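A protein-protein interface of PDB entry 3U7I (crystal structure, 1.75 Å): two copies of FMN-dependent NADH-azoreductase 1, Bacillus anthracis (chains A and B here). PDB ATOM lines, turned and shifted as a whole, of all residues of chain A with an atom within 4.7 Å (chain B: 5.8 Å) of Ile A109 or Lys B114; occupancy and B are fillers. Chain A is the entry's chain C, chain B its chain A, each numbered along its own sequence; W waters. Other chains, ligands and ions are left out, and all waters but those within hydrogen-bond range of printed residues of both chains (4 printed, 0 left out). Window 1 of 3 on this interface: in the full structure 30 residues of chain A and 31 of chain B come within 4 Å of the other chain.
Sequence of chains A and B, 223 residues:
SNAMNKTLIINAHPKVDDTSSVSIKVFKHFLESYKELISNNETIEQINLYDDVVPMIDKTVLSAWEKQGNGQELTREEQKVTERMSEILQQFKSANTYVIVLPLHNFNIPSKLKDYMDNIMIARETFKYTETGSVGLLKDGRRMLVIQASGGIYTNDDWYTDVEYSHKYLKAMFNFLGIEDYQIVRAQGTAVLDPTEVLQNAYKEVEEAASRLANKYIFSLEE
Asn A108 touches Tyr B169, and with the chains exchanged Tyr A169 touches Asn B108. Ile A109 touches Lys B114, and with the chains exchanged Lys A114 touches Ile B109. Ser A111 touches its own counterpart, Ser B111. Ser A111 touches Lys B114, and with the chains exchanged Lys A114 touches Ser B111. Of the 16 pairs that touch across the chains among the printed residues, 10 have their exchanged pair printed and touching as well.
The side-chain carboxylate (OD1) of Asp B118 sits at hydrogen-bond distance from the side-chain amide nitrogen (ND2) of Asn A106, at 2.9 Å. ND2 of Asn B108 lies within hydrogen-bond range of OD1 of Asn A108, 3.0 Å away. The side-chain hydroxyl of Tyr B169 is in hydrogen-bond range of the backbone carbonyl oxygen of Asn A106 (2.7 Å). OD1 of Asp B115 sits at hydrogen-bond distance from OG of Ser A111 (2.7 Å). O of His A105 sits at hydrogen-bond distance from NZ of Lys B114 (3.0 Å).
OD2 of Asp B115 lies within salt-bridge range of NZ of Lys B112. NZ of Lys B114 is in salt-bridge range of OD1 of Asp B118 (2.8 Å). The side-chain amide nitrogen (ND2) of Asn A106 sits close to a ring nitrogen (NE2) of His A105. The backbone carbonyl oxygen (O) of Asp B115 lies within hydrogen-bond range of the side-chain amide nitrogen (ND2) of Asn B119.
Among the printed residues, pairs that only touch across the chains: His A105 with Asp B118 (3.9 Å), Asn A106 with Met B117 (3.98 Å), Asn A108 with Lys B114 (3.7 Å), Asn A108 with Tyr B169 (3.4 Å), Ile A109 with Lys B114 (3.4 Å), Ser A111 with Ser B111 (3.3 Å), Ser A111 with Lys B114 (3.9 Å), Lys A114 with Asn B108 (3.8 Å), Lys A114 with Ile B109 (3.5 Å), Lys A114 with Ser B111 (3.9 Å) and Tyr A169 with Asn B108 (3.5 Å).
Water W4 lies within hydrogen-bond range of OD2 of Asp B115 (2.7 Å) and OG of Ser A111 (3.1 Å). Water W3 lies within hydrogen-bond range of the side-chain carboxylate (OD2) of Asp B118 (2.7 Å), the side-chain amino group (NZ) of Lys B114 (2.8 Å) and the backbone NH (N) of Ser A111 (3.1 Å). Water W2 lies within hydrogen-bond range of the backbone carbonyl oxygen of Asp B118 (2.7 Å), a ring nitrogen (NE2) of His A105 (2.8 Å) and the side-chain amide nitrogen of Asn A106 (3.0 Å). Water W1 lies within hydrogen-bond range of NZ of Lys A114 (2.9 Å) and N of Ser B111 (3.1 Å).
Ile A109 touches just one residue of chain B: Lys B114. Printed residues of chain B within 4 Å of Tyr A169: Asn B108 (3.5 Å). Of the printed residues of chain B, Asn A108 touches Asn B108 (3.0 Å), Lys B114 (3.7 Å) and Tyr B169 (3.4 Å). Leu A102 touches none of the printed residues of chain B. Pro A110 touches none of the printed residues of chain B. The nearest residue of chain B that does not touch Ile A109 is Asn B108 (4.3 Å). The nearest printed residue of chain A that does not touch Met B117 is His A105 (6.6 Å).
Of the 13 printed residues of chain A, 7 touch a printed residue of chain B. Hydrophobic or aromatic side chains of chain A that line the printed part of chain B: His A105 and Tyr A169. Along chain A the printed residues that touch a printed residue of chain B span positions 105 to 169. Of the 13 printed residues of chain B, 8 touch a printed residue of chain A. Hydrophobic or aromatic side chains of chain B within 4 Å of the printed part of chain A: Tyr B169. Among the printed residues, no Asp or Glu carboxylate lies within 4 Å of a Lys or Arg side-chain nitrogen of the other chain.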
ATOM      1  N   LEU A 102      22.250   0.887  -1.953  1.00  0.00           N
ATOM      2  CA  LEU A 102      21.209   1.278  -2.897  1.00  0.00           C
ATOM      3  C   LEU A 102      21.393   0.648  -4.258  1.00  0.00           C
ATOM      4  O   LEU A 102      22.527   0.402  -4.691  1.00  0.00           O
ATOM      5  CB  LEU A 102      21.169   2.799  -3.070  1.00  0.00           C
ATOM      6  CG  LEU A 102      22.322   3.428  -3.857  1.00  0.00           C
ATOM      7  CD1 LEU A 102      21.941   4.817  -4.373  1.00  0.00           C
ATOM      8  CD2 LEU A 102      23.575   3.480  -2.987  1.00  0.00           C
ATOM      9  N   HIS A 105      18.615   3.429  -9.807  1.00  0.00           N
ATOM     10  CA  HIS A 105      17.563   3.431 -10.811  1.00  0.00           C
ATOM     11  C   HIS A 105      17.293   4.856 -11.247  1.00  0.00           C
ATOM     12  O   HIS A 105      17.064   5.735 -10.412  1.00  0.00           O
ATOM     13  CB  HIS A 105      16.278   2.789 -10.288  1.00  0.00           C
ATOM     14  CG  HIS A 105      15.288   2.476 -11.371  1.00  0.00           C
ATOM     15  ND1 HIS A 105      15.640   1.826 -12.537  1.00  0.00           N
ATOM     16  CD2 HIS A 105      13.962   2.736 -11.472  1.00  0.00           C
ATOM     17  CE1 HIS A 105      14.571   1.693 -13.306  1.00  0.00           C
ATOM     18  NE2 HIS A 105      13.539   2.233 -12.681  1.00  0.00           N
ATOM     19  N   ASN A 106      17.333   5.082 -12.557  1.00  0.00           N
ATOM     20  CA  ASN A 106      17.066   6.402 -13.124  1.00  0.00           C
ATOM     21  C   ASN A 106      17.990   7.520 -12.608  1.00  0.00           C
ATOM     22  O   ASN A 106      17.562   8.657 -12.404  1.00  0.00           O
ATOM     23  CB  ASN A 106      15.585   6.740 -12.966  1.00  0.00           C
ATOM     24  CG  ASN A 106      14.707   5.771 -13.727  1.00  0.00           C
ATOM     25  OD1 ASN A 106      15.087   5.297 -14.798  1.00  0.00           O
ATOM     26  ND2 ASN A 106      13.545   5.449 -13.170  1.00  0.00           N
ATOM     27  N   ASN A 108      19.580   8.613  -9.998  1.00  0.00           N
ATOM     28  CA  ASN A 108      19.493   9.415  -8.766  1.00  0.00           C
ATOM     29  C   ASN A 108      19.251   8.498  -7.580  1.00  0.00           C
ATOM     30  O   ASN A 108      18.990   7.305  -7.758  1.00  0.00           O
ATOM     31  CB  ASN A 108      18.363  10.456  -8.857  1.00  0.00           C
ATOM     32  CG  ASN A 108      18.699  11.778  -8.153  1.00  0.00           C
ATOM     33  OD1 ASN A 108      19.409  11.815  -7.132  1.00  0.00           O
ATOM     34  ND2 ASN A 108      18.168  12.878  -8.698  1.00  0.00           N
ATOM     35  N   ILE A 109      19.334   9.051  -6.374  1.00  0.00           N
ATOM     36  CA  ILE A 109      19.063   8.279  -5.173  1.00  0.00           C
ATOM     37  C   ILE A 109      17.592   7.843  -5.147  1.00  0.00           C
ATOM     38  O   ILE A 109      16.723   8.547  -5.679  1.00  0.00           O
ATOM     39  CB  ILE A 109      19.407   9.079  -3.898  1.00  0.00           C
ATOM     40  CG1 ILE A 109      18.515  10.332  -3.780  1.00  0.00           C
ATOM     41  CG2 ILE A 109      20.892   9.450  -3.899  1.00  0.00           C
ATOM     42  CD1 ILE A 109      18.684  11.096  -2.476  1.00  0.00           C
ATOM     43  N   PRO A 110      17.311   6.665  -4.553  1.00  0.00           N
ATOM     44  CA  PRO A 110      15.924   6.233  -4.359  1.00  0.00           C
ATOM     45  C   PRO A 110      15.096   7.307  -3.652  1.00  0.00           C
ATOM     46  O   PRO A 110      15.602   8.008  -2.778  1.00  0.00           O
ATOM     47  CB  PRO A 110      16.072   4.997  -3.464  1.00  0.00           C
ATOM     48  CG  PRO A 110      17.395   4.438  -3.823  1.00  0.00           C
ATOM     49  CD  PRO A 110      18.273   5.647  -4.078  1.00  0.00           C
ATOM     50  N   SER A 111      13.823   7.422  -4.018  1.00  0.00           N
ATOM     51  CA  SER A 111      12.942   8.408  -3.389  1.00  0.00           C
ATOM     52  C   SER A 111      13.003   8.374  -1.862  1.00  0.00           C
ATOM     53  O   SER A 111      13.029   9.424  -1.219  1.00  0.00           O
ATOM     54  CB  SER A 111      11.503   8.232  -3.861  1.00  0.00           C
ATOM     55  OG  SER A 111      11.049   6.919  -3.609  1.00  0.00           O
ATOM     56  N   LEU A 113      15.475   7.497  -0.021  1.00  0.00           N
ATOM     57  CA  LEU A 113      16.760   8.043   0.438  1.00  0.00           C
ATOM     58  C   LEU A 113      16.719   9.580   0.463  1.00  0.00           C
ATOM     59  O   LEU A 113      17.338  10.216   1.322  1.00  0.00           O
ATOM     60  CB  LEU A 113      17.935   7.530  -0.408  1.00  0.00           C
ATOM     61  CG  LEU A 113      19.341   7.900   0.067  1.00  0.00           C
ATOM     62  CD1 LEU A 113      19.522   7.589   1.551  1.00  0.00           C
ATOM     63  CD2 LEU A 113      20.408   7.185  -0.763  1.00  0.00           C
ATOM     64  N   LYS A 114      15.982  10.174  -0.473  1.00  0.00           N
ATOM     65  CA  LYS A 114      15.707  11.610  -0.403  1.00  0.00           C
ATOM     66  C   LYS A 114      14.931  11.949   0.872  1.00  0.00           C
ATOM     67  O   LYS A 114      15.289  12.895   1.573  1.00  0.00           O
ATOM     68  CB  LYS A 114      14.950  12.106  -1.641  1.00  0.00           C
ATOM     69  CG  LYS A 114      14.701  13.620  -1.641  1.00  0.00           C
ATOM     70  CD  LYS A 114      15.968  14.394  -1.249  1.00  0.00           C
ATOM     71  CE  LYS A 114      15.877  15.906  -1.551  1.00  0.00           C
ATOM     72  NZ  LYS A 114      14.703  16.591  -0.945  1.00  0.00           N
ATOM     73  N   MET A 117      17.317  11.887   3.653  1.00  0.00           N
ATOM     74  CA  MET A 117      18.130  13.100   3.675  1.00  0.00           C
ATOM     75  C   MET A 117      17.328  14.227   4.313  1.00  0.00           C
ATOM     76  O   MET A 117      17.879  15.047   5.041  1.00  0.00           O
ATOM     77  CB  MET A 117      18.593  13.514   2.267  1.00  0.00           C
ATOM     78  CG  MET A 117      19.465  12.480   1.533  1.00  0.00           C
ATOM     79  SD  MET A 117      21.065  11.992   2.515  1.00  0.00           S
ATOM     80  CE  MET A 117      21.843  13.786   2.690  1.00  0.00           C
ATOM     81  N   SER A 166      23.188  10.005  -8.206  1.00  0.00           N
ATOM     82  CA  SER A 166      23.174   9.308  -6.927  1.00  0.00           C
ATOM     83  C   SER A 166      24.481   9.600  -6.168  1.00  0.00           C
ATOM     84  O   SER A 166      24.467  10.209  -5.090  1.00  0.00           O
ATOM     85  CB  SER A 166      23.008   7.797  -7.143  1.00  0.00           C
ATOM     86  OG  SER A 166      24.031   7.273  -7.979  1.00  0.00           O
ATOM     87  N   TYR A 169      25.428  13.499  -5.689  1.00  0.00           N
ATOM     88  CA  TYR A 169      24.639  14.090  -4.621  1.00  0.00           C
ATOM     89  C   TYR A 169      25.097  13.605  -3.251  1.00  0.00           C
ATOM     90  O   TYR A 169      25.377  14.416  -2.364  1.00  0.00           O
ATOM     91  CB  TYR A 169      23.163  13.781  -4.826  1.00  0.00           C
ATOM     92  CG  TYR A 169      22.264  14.291  -3.733  1.00  0.00           C
ATOM     93  CD1 TYR A 169      21.931  15.636  -3.658  1.00  0.00           C
ATOM     94  CD2 TYR A 169      21.742  13.431  -2.780  1.00  0.00           C
ATOM     95  CE1 TYR A 169      21.100  16.111  -2.666  1.00  0.00           C
ATOM     96  CE2 TYR A 169      20.910  13.895  -1.779  1.00  0.00           C
ATOM     97  CZ  TYR A 169      20.588  15.235  -1.723  1.00  0.00           C
ATOM     98  OH  TYR A 169      19.745  15.708  -0.734  1.00  0.00           O
ATOM     99  N   LEU A 170      25.191  12.292  -3.065  1.00  0.00           N
ATOM    100  CA  LEU A 170      25.584  11.769  -1.751  1.00  0.00           C
ATOM    101  C   LEU A 170      26.950  12.274  -1.281  1.00  0.00           C
ATOM    102  O   LEU A 170      27.076  12.724  -0.143  1.00  0.00           O
ATOM    103  CB  LEU A 170      25.509  10.236  -1.703  1.00  0.00           C
ATOM    104  CG  LEU A 170      24.095   9.656  -1.804  1.00  0.00           C
ATOM    105  CD1 LEU A 170      24.132   8.146  -1.952  1.00  0.00           C
ATOM    106  CD2 LEU A 170      23.265  10.063  -0.594  1.00  0.00           C
ATOM    107  N   ASN B 108      18.150  18.787  -4.234  1.00  0.00           N
ATOM    108  CA  ASN B 108      17.775  17.725  -5.164  1.00  0.00           C
ATOM    109  C   ASN B 108      16.271  17.796  -5.398  1.00  0.00           C
ATOM    110  O   ASN B 108      15.574  18.555  -4.720  1.00  0.00           O
ATOM    111  CB  ASN B 108      18.182  16.349  -4.601  1.00  0.00           C
ATOM    112  CG  ASN B 108      18.462  15.307  -5.689  1.00  0.00           C
ATOM    113  OD1 ASN B 108      18.012  15.431  -6.836  1.00  0.00           O
ATOM    114  ND2 ASN B 108      19.201  14.261  -5.323  1.00  0.00           N
ATOM    115  N   ILE B 109      15.773  17.027  -6.365  1.00  0.00           N
ATOM    116  CA  ILE B 109      14.336  16.973  -6.619  1.00  0.00           C
ATOM    117  C   ILE B 109      13.576  16.428  -5.402  1.00  0.00           C
ATOM    118  O   ILE B 109      14.119  15.651  -4.617  1.00  0.00           O
ATOM    119  CB  ILE B 109      14.006  16.121  -7.872  1.00  0.00           C
ATOM    120  CG1 ILE B 109      14.555  14.695  -7.714  1.00  0.00           C
ATOM    121  CG2 ILE B 109      14.549  16.787  -9.136  1.00  0.00           C
ATOM    122  CD1 ILE B 109      14.113  13.744  -8.810  1.00  0.00           C
ATOM    123  N   PRO B 110      12.318  16.857  -5.225  1.00  0.00           N
ATOM    124  CA  PRO B 110      11.475  16.295  -4.171  1.00  0.00           C
ATOM    125  C   PRO B 110      11.313  14.788  -4.348  1.00  0.00           C
ATOM    126  O   PRO B 110      11.304  14.305  -5.483  1.00  0.00           O
ATOM    127  CB  PRO B 110      10.131  17.003  -4.390  1.00  0.00           C
ATOM    128  CG  PRO B 110      10.504  18.304  -5.033  1.00  0.00           C
ATOM    129  CD  PRO B 110      11.643  17.951  -5.945  1.00  0.00           C
ATOM    130  N   SER B 111      11.173  14.060  -3.243  1.00  0.00           N
ATOM    131  CA  SER B 111      11.074  12.600  -3.310  1.00  0.00           C
ATOM    132  C   SER B 111       9.937  12.101  -4.226  1.00  0.00           C
ATOM    133  O   SER B 111      10.105  11.111  -4.948  1.00  0.00           O
ATOM    134  CB  SER B 111      10.987  11.985  -1.907  1.00  0.00           C
ATOM    135  OG  SER B 111       9.789  12.360  -1.256  1.00  0.00           O
ATOM    136  N   LYS B 112       8.791  12.775  -4.211  1.00  0.00           N
ATOM    137  CA  LYS B 112       7.697  12.385  -5.108  1.00  0.00           C
ATOM    138  C   LYS B 112       7.994  12.675  -6.583  1.00  0.00           C
ATOM    139  O   LYS B 112       7.410  12.030  -7.468  1.00  0.00           O
ATOM    140  CB  LYS B 112       6.352  13.010  -4.694  1.00  0.00           C
ATOM    141  CG  LYS B 112       5.752  12.463  -3.392  1.00  0.00           C
ATOM    142  CD  LYS B 112       5.733  10.928  -3.336  1.00  0.00           C
ATOM    143  CE  LYS B 112       4.821  10.295  -4.387  1.00  0.00           C
ATOM    144  NZ  LYS B 112       4.712   8.794  -4.222  1.00  0.00           N
ATOM    145  N   LEU B 113       8.891  13.632  -6.859  1.00  0.00           N
ATOM    146  CA  LEU B 113       9.305  13.878  -8.241  1.00  0.00           C
ATOM    147  C   LEU B 113      10.198  12.732  -8.745  1.00  0.00           C
ATOM    148  O   LEU B 113      10.096  12.321  -9.907  1.00  0.00           O
ATOM    149  CB  LEU B 113       9.958  15.267  -8.427  1.00  0.00           C
ATOM    150  CG  LEU B 113      10.276  15.736  -9.867  1.00  0.00           C
ATOM    151  CD1 LEU B 113       9.066  15.612 -10.810  1.00  0.00           C
ATOM    152  CD2 LEU B 113      10.888  17.160  -9.931  1.00  0.00           C
ATOM    153  N   LYS B 114      11.045  12.192  -7.875  1.00  0.00           N
ATOM    154  CA  LYS B 114      11.772  10.964  -8.218  1.00  0.00           C
ATOM    155  C   LYS B 114      10.821   9.799  -8.530  1.00  0.00           C
ATOM    156  O   LYS B 114      11.044   9.076  -9.499  1.00  0.00           O
ATOM    157  CB  LYS B 114      12.749  10.545  -7.115  1.00  0.00           C
ATOM    158  CG  LYS B 114      13.522   9.255  -7.435  1.00  0.00           C
ATOM    159  CD  LYS B 114      14.396   9.405  -8.694  1.00  0.00           C
ATOM    160  CE  LYS B 114      15.413   8.268  -8.844  1.00  0.00           C
ATOM    161  NZ  LYS B 114      14.845   6.887  -8.845  1.00  0.00           N
ATOM    162  N   ASP B 115       9.774   9.616  -7.717  1.00  0.00           N
ATOM    163  CA  ASP B 115       8.775   8.578  -7.988  1.00  0.00           C
ATOM    164  C   ASP B 115       8.140   8.817  -9.360  1.00  0.00           C
ATOM    165  O   ASP B 115       7.920   7.874 -10.124  1.00  0.00           O
ATOM    166  CB  ASP B 115       7.677   8.557  -6.926  1.00  0.00           C
ATOM    167  CG  ASP B 115       8.164   8.041  -5.578  1.00  0.00           C
ATOM    168  OD1 ASP B 115       9.226   7.376  -5.531  1.00  0.00           O
ATOM    169  OD2 ASP B 115       7.464   8.287  -4.567  1.00  0.00           O
ATOM    170  N   TYR B 116       7.844  10.078  -9.670  1.00  0.00           N
ATOM    171  CA  TYR B 116       7.306  10.419 -10.990  1.00  0.00           C
ATOM    172  C   TYR B 116       8.287  10.044 -12.120  1.00  0.00           C
ATOM    173  O   TYR B 116       7.879   9.489 -13.150  1.00  0.00           O
ATOM    174  CB  TYR B 116       6.920  11.910 -11.069  1.00  0.00           C
ATOM    175  CG  TYR B 116       6.194  12.265 -12.356  1.00  0.00           C
ATOM    176  CD1 TYR B 116       4.833  11.997 -12.516  1.00  0.00           C
ATOM    177  CD2 TYR B 116       6.869  12.852 -13.415  1.00  0.00           C
ATOM    178  CE1 TYR B 116       4.170  12.317 -13.699  1.00  0.00           C
ATOM    179  CE2 TYR B 116       6.216  13.169 -14.601  1.00  0.00           C
ATOM    180  CZ  TYR B 116       4.871  12.905 -14.744  1.00  0.00           C
ATOM    181  OH  TYR B 116       4.237  13.228 -15.936  1.00  0.00           O
ATOM    182  N   MET B 117       9.569  10.354 -11.938  1.00  0.00           N
ATOM    183  CA  MET B 117      10.576   9.982 -12.930  1.00  0.00           C
ATOM    184  C   MET B 117      10.562   8.464 -13.140  1.00  0.00           C
ATOM    185  O   MET B 117      10.684   7.982 -14.274  1.00  0.00           O
ATOM    186  CB  MET B 117      11.976  10.437 -12.495  1.00  0.00           C
ATOM    187  CG  MET B 117      12.128  11.949 -12.291  1.00  0.00           C
ATOM    188  SD  MET B 117      11.650  12.964 -13.890  1.00  0.00           S
ATOM    189  CE  MET B 117      13.050  12.258 -15.067  1.00  0.00           C
ATOM    190  N   ASP B 118      10.403   7.725 -12.039  1.00  0.00           N
ATOM    191  CA  ASP B 118      10.370   6.258 -12.062  1.00  0.00           C
ATOM    192  C   ASP B 118       9.155   5.709 -12.822  1.00  0.00           C
ATOM    193  O   ASP B 118       9.167   4.569 -13.284  1.00  0.00           O
ATOM    194  CB  ASP B 118      10.411   5.685 -10.639  1.00  0.00           C
ATOM    195  CG  ASP B 118      11.730   5.952  -9.930  1.00  0.00           C
ATOM    196  OD1 ASP B 118      12.733   6.352 -10.578  1.00  0.00           O
ATOM    197  OD2 ASP B 118      11.767   5.744  -8.700  1.00  0.00           O
ATOM    198  N   ASN B 119       8.115   6.527 -12.941  1.00  0.00           N
ATOM    199  CA  ASN B 119       6.921   6.172 -13.704  1.00  0.00           C
ATOM    200  C   ASN B 119       7.060   6.487 -15.194  1.00  0.00           C
ATOM    201  O   ASN B 119       6.472   5.802 -16.038  1.00  0.00           O
ATOM    202  CB  ASN B 119       5.703   6.932 -13.164  1.00  0.00           C
ATOM    203  CG  ASN B 119       5.050   6.246 -11.979  1.00  0.00           C
ATOM    204  OD1 ASN B 119       3.979   5.649 -12.111  1.00  0.00           O
ATOM    205  ND2 ASN B 119       5.670   6.354 -10.812  1.00  0.00           N
ATOM    206  N   TYR B 169      19.942  17.291 -12.644  1.00  0.00           N
ATOM    207  CA  TYR B 169      19.282  16.018 -12.911  1.00  0.00           C
ATOM    208  C   TYR B 169      18.159  16.167 -13.939  1.00  0.00           C
ATOM    209  O   TYR B 169      18.128  15.444 -14.940  1.00  0.00           O
ATOM    210  CB  TYR B 169      18.737  15.403 -11.627  1.00  0.00           C
ATOM    211  CG  TYR B 169      17.942  14.122 -11.839  1.00  0.00           C
ATOM    212  CD1 TYR B 169      18.586  12.909 -12.064  1.00  0.00           C
ATOM    213  CD2 TYR B 169      16.552  14.128 -11.812  1.00  0.00           C
ATOM    214  CE1 TYR B 169      17.861  11.733 -12.251  1.00  0.00           C
ATOM    215  CE2 TYR B 169      15.822  12.963 -11.994  1.00  0.00           C
ATOM    216  CZ  TYR B 169      16.476  11.768 -12.213  1.00  0.00           C
ATOM    217  OH  TYR B 169      15.741  10.607 -12.400  1.00  0.00           O
HETATM  218  O   HOH W   1      11.898  15.735  -0.729  1.00  0.00           O
HETATM  219  O   HOH W   2      11.497   3.478 -14.177  1.00  0.00           O
HETATM  220  O   HOH W   3      13.522   5.866  -6.625  1.00  0.00           O
HETATM  221  O   HOH W   4       8.465   7.826  -2.115  1.00  0.00           O
